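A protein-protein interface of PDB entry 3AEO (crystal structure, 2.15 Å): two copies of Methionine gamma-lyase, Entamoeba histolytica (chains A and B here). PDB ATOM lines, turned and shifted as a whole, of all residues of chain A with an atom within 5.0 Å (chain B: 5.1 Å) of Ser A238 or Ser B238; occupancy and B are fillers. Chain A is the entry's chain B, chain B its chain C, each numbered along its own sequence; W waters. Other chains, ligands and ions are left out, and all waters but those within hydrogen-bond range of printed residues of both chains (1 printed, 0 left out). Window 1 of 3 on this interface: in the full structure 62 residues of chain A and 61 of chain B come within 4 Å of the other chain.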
ATOM      1  N   ALA A  79     -21.467  -8.135 -21.553  1.00  0.00           N
ATOM      2  CA  ALA A  79     -21.632  -8.983 -20.377  1.00  0.00           C
ATOM      3  C   ALA A  79     -22.422  -8.231 -19.309  1.00  0.00           C
ATOM      4  O   ALA A  79     -22.302  -6.995 -19.187  1.00  0.00           O
ATOM      5  CB  ALA A  79     -20.234  -9.394 -19.795  1.00  0.00           C
ATOM      6  N   PHE A  80     -23.195  -8.979 -18.526  1.00  0.00           N
ATOM      7  CA  PHE A  80     -24.049  -8.400 -17.494  1.00  0.00           C
ATOM      8  C   PHE A  80     -23.902  -9.165 -16.181  1.00  0.00           C
ATOM      9  O   PHE A  80     -23.288 -10.257 -16.145  1.00  0.00           O
ATOM     10  CB  PHE A  80     -25.514  -8.455 -17.965  1.00  0.00           C
ATOM     11  CG  PHE A  80     -25.762  -7.688 -19.235  1.00  0.00           C
ATOM     12  CD1 PHE A  80     -26.187  -6.364 -19.184  1.00  0.00           C
ATOM     13  CD2 PHE A  80     -25.558  -8.285 -20.482  1.00  0.00           C
ATOM     14  CE1 PHE A  80     -26.419  -5.653 -20.368  1.00  0.00           C
ATOM     15  CE2 PHE A  80     -25.775  -7.596 -21.642  1.00  0.00           C
ATOM     16  CZ  PHE A  80     -26.210  -6.260 -21.594  1.00  0.00           C
ATOM     17  N   GLY A  81     -24.449  -8.580 -15.113  1.00  0.00           N
ATOM     18  CA  GLY A  81     -24.543  -9.219 -13.779  1.00  0.00           C
ATOM     19  C   GLY A  81     -25.401 -10.486 -13.714  1.00  0.00           C
ATOM     20  O   GLY A  81     -25.333 -11.217 -12.741  1.00  0.00           O
ATOM     21  N   SER A  82     -26.200 -10.758 -14.741  1.00  0.00           N
ATOM     22  CA  SER A  82     -27.047 -11.956 -14.764  1.00  0.00           C
ATOM     23  C   SER A  82     -27.649 -12.102 -16.143  1.00  0.00           C
ATOM     24  O   SER A  82     -27.631 -11.148 -16.939  1.00  0.00           O
ATOM     25  CB  SER A  82     -28.183 -11.876 -13.728  1.00  0.00           C
ATOM     26  OG  SER A  82     -29.009 -10.757 -13.979  1.00  0.00           O
ATOM     27  N   GLY A  85     -30.314  -9.550 -16.578  1.00  0.00           N
ATOM     28  CA  GLY A  85     -29.751  -8.273 -17.043  1.00  0.00           C
ATOM     29  C   GLY A  85     -29.518  -8.250 -18.569  1.00  0.00           C
ATOM     30  O   GLY A  85     -29.796  -7.240 -19.237  1.00  0.00           O
ATOM     31  N   ARG A 233     -26.999  -0.410 -20.788  1.00  0.00           N
ATOM     32  CA  ARG A 233     -26.317  -1.010 -19.646  1.00  0.00           C
ATOM     33  C   ARG A 233     -25.677   0.062 -18.765  1.00  0.00           C
ATOM     34  O   ARG A 233     -25.649  -0.079 -17.526  1.00  0.00           O
ATOM     35  CB  ARG A 233     -25.254  -2.031 -20.113  1.00  0.00           C
ATOM     36  CG  ARG A 233     -24.537  -2.793 -18.998  1.00  0.00           C
ATOM     37  CD  ARG A 233     -23.469  -3.739 -19.510  1.00  0.00           C
ATOM     38  NE  ARG A 233     -22.377  -2.994 -20.131  1.00  0.00           N
ATOM     39  CZ  ARG A 233     -21.291  -3.515 -20.707  1.00  0.00           C
ATOM     40  NH1 ARG A 233     -20.388  -2.688 -21.228  1.00  0.00           N
ATOM     41  NH2 ARG A 233     -21.069  -4.833 -20.737  1.00  0.00           N
ATOM     42  N   ALA A 236     -28.767   1.437 -16.878  1.00  0.00           N
ATOM     43  CA  ALA A 236     -29.447   0.406 -16.099  1.00  0.00           C
ATOM     44  C   ALA A 236     -28.523  -0.270 -15.066  1.00  0.00           C
ATOM     45  O   ALA A 236     -28.971  -0.670 -14.006  1.00  0.00           O
ATOM     46  CB  ALA A 236     -30.058  -0.619 -17.010  1.00  0.00           C
ATOM     47  N   GLY A 237     -27.240  -0.412 -15.376  1.00  0.00           N
ATOM     48  CA  GLY A 237     -26.253  -0.822 -14.353  1.00  0.00           C
ATOM     49  C   GLY A 237     -26.119  -2.296 -13.999  1.00  0.00           C
ATOM     50  O   GLY A 237     -25.610  -2.627 -12.896  1.00  0.00           O
ATOM     51  N   SER A 238     -26.573  -3.186 -14.889  1.00  0.00           N
ATOM     52  CA  SER A 238     -26.305  -4.621 -14.716  1.00  0.00           C
ATOM     53  C   SER A 238     -24.923  -4.959 -15.303  1.00  0.00           C
ATOM     54  O   SER A 238     -24.769  -5.145 -16.513  1.00  0.00           O
ATOM     55  CB  SER A 238     -27.402  -5.499 -15.320  1.00  0.00           C
ATOM     56  OG  SER A 238     -27.128  -6.882 -15.068  1.00  0.00           O
ATOM     57  N   LEU A 239     -23.912  -4.977 -14.432  1.00  0.00           N
ATOM     58  CA  LEU A 239     -22.539  -5.194 -14.844  1.00  0.00           C
ATOM     59  C   LEU A 239     -22.077  -6.572 -14.371  1.00  0.00           C
ATOM     60  O   LEU A 239     -22.450  -6.995 -13.280  1.00  0.00           O
ATOM     61  CB  LEU A 239     -21.627  -4.126 -14.198  1.00  0.00           C
ATOM     62  CG  LEU A 239     -22.086  -2.675 -14.362  1.00  0.00           C
ATOM     63  CD1 LEU A 239     -21.092  -1.776 -13.626  1.00  0.00           C
ATOM     64  CD2 LEU A 239     -22.138  -2.365 -15.867  1.00  0.00           C
ATOM     65  N   MET A 240     -21.246  -7.233 -15.172  1.00  0.00           N
ATOM     66  CA  MET A 240     -20.456  -8.366 -14.715  1.00  0.00           C
ATOM     67  C   MET A 240     -19.219  -7.867 -13.938  1.00  0.00           C
ATOM     68  O   MET A 240     -18.444  -7.044 -14.460  1.00  0.00           O
ATOM     69  CB  MET A 240     -20.019  -9.200 -15.928  1.00  0.00           C
ATOM     70  CG  MET A 240     -19.140 -10.418 -15.538  1.00  0.00           C
ATOM     71  SD  MET A 240     -18.819 -11.510 -16.922  1.00  0.00           S
ATOM     72  CE  MET A 240     -20.356 -12.432 -17.156  1.00  0.00           C
ATOM     73  N   ALA B  79     -28.518  -4.624  -2.371  1.00  0.00           N
ATOM     74  CA  ALA B  79     -27.258  -4.331  -3.037  1.00  0.00           C
ATOM     75  C   ALA B  79     -27.395  -4.526  -4.563  1.00  0.00           C
ATOM     76  O   ALA B  79     -28.147  -5.423  -4.994  1.00  0.00           O
ATOM     77  CB  ALA B  79     -26.183  -5.283  -2.496  1.00  0.00           C
ATOM     78  N   PHE B  80     -26.607  -3.804  -5.352  1.00  0.00           N
ATOM     79  CA  PHE B  80     -26.676  -3.866  -6.832  1.00  0.00           C
ATOM     80  C   PHE B  80     -25.271  -3.860  -7.426  1.00  0.00           C
ATOM     81  O   PHE B  80     -24.317  -3.491  -6.744  1.00  0.00           O
ATOM     82  CB  PHE B  80     -27.439  -2.637  -7.394  1.00  0.00           C
ATOM     83  CG  PHE B  80     -28.874  -2.549  -6.929  1.00  0.00           C
ATOM     84  CD1 PHE B  80     -29.899  -3.099  -7.690  1.00  0.00           C
ATOM     85  CD2 PHE B  80     -29.190  -1.967  -5.714  1.00  0.00           C
ATOM     86  CE1 PHE B  80     -31.222  -3.074  -7.226  1.00  0.00           C
ATOM     87  CE2 PHE B  80     -30.524  -1.891  -5.250  1.00  0.00           C
ATOM     88  CZ  PHE B  80     -31.531  -2.447  -6.006  1.00  0.00           C
ATOM     89  N   GLY B  81     -25.177  -4.177  -8.720  1.00  0.00           N
ATOM     90  CA  GLY B  81     -23.917  -4.183  -9.477  1.00  0.00           C
ATOM     91  C   GLY B  81     -23.331  -2.791  -9.693  1.00  0.00           C
ATOM     92  O   GLY B  81     -22.160  -2.668 -10.092  1.00  0.00           O
ATOM     93  N   SER B  82     -24.131  -1.746  -9.457  1.00  0.00           N
ATOM     94  CA  SER B  82     -23.643  -0.363  -9.622  1.00  0.00           C
ATOM     95  C   SER B  82     -24.619   0.610  -8.971  1.00  0.00           C
ATOM     96  O   SER B  82     -25.786   0.286  -8.765  1.00  0.00           O
ATOM     97  CB  SER B  82     -23.475  -0.010 -11.118  1.00  0.00           C
ATOM     98  OG  SER B  82     -24.724  -0.057 -11.790  1.00  0.00           O
ATOM     99  N   GLY B  85     -27.482   0.969 -11.007  1.00  0.00           N
ATOM    100  CA  GLY B  85     -28.361  -0.166 -10.800  1.00  0.00           C
ATOM    101  C   GLY B  85     -29.309   0.153  -9.647  1.00  0.00           C
ATOM    102  O   GLY B  85     -30.491  -0.142  -9.718  1.00  0.00           O
ATOM    103  N   ARG B 233     -35.305  -5.879  -8.948  1.00  0.00           N
ATOM    104  CA  ARG B 233     -33.927  -6.329  -9.102  1.00  0.00           C
ATOM    105  C   ARG B 233     -33.831  -7.723  -9.708  1.00  0.00           C
ATOM    106  O   ARG B 233     -32.981  -7.970 -10.568  1.00  0.00           O
ATOM    107  CB  ARG B 233     -33.167  -6.290  -7.759  1.00  0.00           C
ATOM    108  CG  ARG B 233     -31.708  -6.731  -7.877  1.00  0.00           C
ATOM    109  CD  ARG B 233     -30.988  -6.684  -6.526  1.00  0.00           C
ATOM    110  NE  ARG B 233     -31.497  -7.728  -5.641  1.00  0.00           N
ATOM    111  CZ  ARG B 233     -31.140  -7.920  -4.368  1.00  0.00           C
ATOM    112  NH1 ARG B 233     -31.704  -8.920  -3.684  1.00  0.00           N
ATOM    113  NH2 ARG B 233     -30.225  -7.127  -3.780  1.00  0.00           N
ATOM    114  N   ALA B 236     -34.612  -7.187 -13.370  1.00  0.00           N
ATOM    115  CA  ALA B 236     -33.716  -6.279 -14.109  1.00  0.00           C
ATOM    116  C   ALA B 236     -32.265  -6.776 -14.048  1.00  0.00           C
ATOM    117  O   ALA B 236     -31.436  -6.448 -14.913  1.00  0.00           O
ATOM    118  CB  ALA B 236     -33.829  -4.895 -13.592  1.00  0.00           C
ATOM    119  N   GLY B 237     -31.965  -7.564 -13.018  1.00  0.00           N
ATOM    120  CA  GLY B 237     -30.734  -8.324 -12.984  1.00  0.00           C
ATOM    121  C   GLY B 237     -29.462  -7.568 -12.632  1.00  0.00           C
ATOM    122  O   GLY B 237     -28.366  -8.041 -12.971  1.00  0.00           O
ATOM    123  N   SER B 238     -29.567  -6.418 -11.956  1.00  0.00           N
ATOM    124  CA  SER B 238     -28.347  -5.721 -11.515  1.00  0.00           C
ATOM    125  C   SER B 238     -27.921  -6.230 -10.130  1.00  0.00           C
ATOM    126  O   SER B 238     -28.388  -5.751  -9.118  1.00  0.00           O
ATOM    127  CB  SER B 238     -28.485  -4.205 -11.533  1.00  0.00           C
ATOM    128  OG  SER B 238     -27.280  -3.570 -11.066  1.00  0.00           O
ATOM    129  N   LEU B 239     -27.033  -7.222 -10.116  1.00  0.00           N
ATOM    130  CA  LEU B 239     -26.664  -7.931  -8.893  1.00  0.00           C
ATOM    131  C   LEU B 239     -25.305  -7.494  -8.416  1.00  0.00           C
ATOM    132  O   LEU B 239     -24.424  -7.244  -9.233  1.00  0.00           O
ATOM    133  CB  LEU B 239     -26.604  -9.434  -9.183  1.00  0.00           C
ATOM    134  CG  LEU B 239     -27.907 -10.058  -9.646  1.00  0.00           C
ATOM    135  CD1 LEU B 239     -27.656 -11.552  -9.786  1.00  0.00           C
ATOM    136  CD2 LEU B 239     -29.036  -9.751  -8.595  1.00  0.00           C
ATOM    137  N   MET B 240     -25.113  -7.440  -7.113  1.00  0.00           N
ATOM    138  CA  MET B 240     -23.759  -7.322  -6.576  1.00  0.00           C
ATOM    139  C   MET B 240     -23.125  -8.721  -6.554  1.00  0.00           C
ATOM    140  O   MET B 240     -23.693  -9.633  -5.993  1.00  0.00           O
ATOM    141  CB  MET B 240     -23.758  -6.694  -5.161  1.00  0.00           C
ATOM    142  CG  MET B 240     -22.339  -6.594  -4.530  1.00  0.00           C
ATOM    143  SD  MET B 240     -22.320  -5.641  -2.987  1.00  0.00           S
ATOM    144  CE  MET B 240     -22.492  -3.935  -3.609  1.00  0.00           C
HETATM  145  O   HOH W   1     -24.735  -6.442 -11.978  1.00  0.00           O
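OG of Ser A82 is in hydrogen-bond range of O of Gly B237 (3.0 Å). The backbone carbonyl oxygen (O) of Gly A237 sits at hydrogen-bond distance from the side-chain hydroxyl (OG) of Ser B82, at 2.9 Å. The backbone carbonyl oxygen (O) of Gly A237 is in hydrogen-bond range of the side-chain hydroxyl (OG) of Ser B238 (2.7 Å). O of Gly B237 lies within hydrogen-bond range of OG of Ser A238.
The side-chain hydroxyl of Ser A238 sits at hydrogen-bond distance from the backbone NH of Gly A81 (3.2 Å). The backbone NH of Gly A81 sits close to the backbone carbonyl oxygen of Leu A239. The side-chain hydroxyl (OG) of Ser A82 lies within hydrogen-bond range of the backbone NH (N) of Gly A85, at 3.1 Å. The side-chain hydroxyl (OG) of Ser B238 lies within hydrogen-bond range of the backbone NH (N) of Gly B81 (3.2 Å). N of Gly B81 lies close to O of Leu B239 (3.2 Å). N of Gly B85 sits at hydrogen-bond distance from OG of Ser B82 (3.0 Å).
Among the printed residues, merely in contact across the chains: Gly A85 with Ala B236 (3.3 Å), Ala A236 with Gly B85 (3.3 Å), Gly A81 with Leu B239 (3.8 Å), Leu A239 with Gly B81 (3.8 Å), Gly A85 with Gly B237 (3.8 Å), Ser A238 with Ser B238 (3.9 Å), Leu A239 with Ser B82 (3.9 Å), Gly A81 with Gly B237 (3.9 Å), Gly A237 with Gly B81 (3.9 Å), Gly A237 with Gly B85 (3.99 Å) and Ser A82 with Leu B239 (3.99 Å).
Ser A238 touches just these residues of chain B: Gly B237 (2.7 Å) and Ser B238 (3.9 Å). Ser B238 touches just these residues of chain A: Gly A237 (2.7 Å) and Ser A238 (3.9 Å). Of the printed residues of chain B, Gly A237 touches Gly B81, Ser B82, Gly B85 and Ser B238. Printed residues of chain B within 4 Å of Ser A82: Gly B237 (3.0 Å) and Leu B239 (3.99 Å). Printed residues of chain B within 4 Å of Gly A85: Ala B236 (3.3 Å) and Gly B237 (3.8 Å). Ala A79 touches none of the printed residues of chain B. Arg B233 touches none of the printed residues of chain A. The nearest residue of chain A that does not touch Ser B238 is Ala A236 (4.3 Å).
Printed residues of chain A that touch a printed residue of chain B: Gly A81, Ser A82, Gly A85, Ala A236, Gly A237, Ser A238 and Leu A239. Hydrophobic or aromatic side chains of chain A that line the printed part of chain B: Leu A239. Along chain A the printed residues that touch a printed residue of chain B span positions 81 to 239. Hydrophobic or aromatic side chains of chain B that line the printed part of chain A: Leu B239. Among the printed residues, no Asp or Glu carboxylate lies within 4 Å of a Lys or Arg side-chain nitrogen of the other chain.
Gly A81 touches Gly B237, and with the chains exchanged Gly A237 touches Gly B81. Gly A81 touches Leu B239, and with the chains exchanged Leu A239 touches Gly B81. Gly A85 touches Gly B237, and with the chains exchanged Gly A237 touches Gly B85. Gly A237 touches Ser B238, and with the chains exchanged Ser A238 touches Gly B237. Positions printed for both chains: 79, 80, 81, 82, 85, 233, 236, 237, 238, 239 and 240.
Water W1 bridges the backbone carbonyl oxygen of Leu A239 and the backbone carbonyl oxygen of Leu B239.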
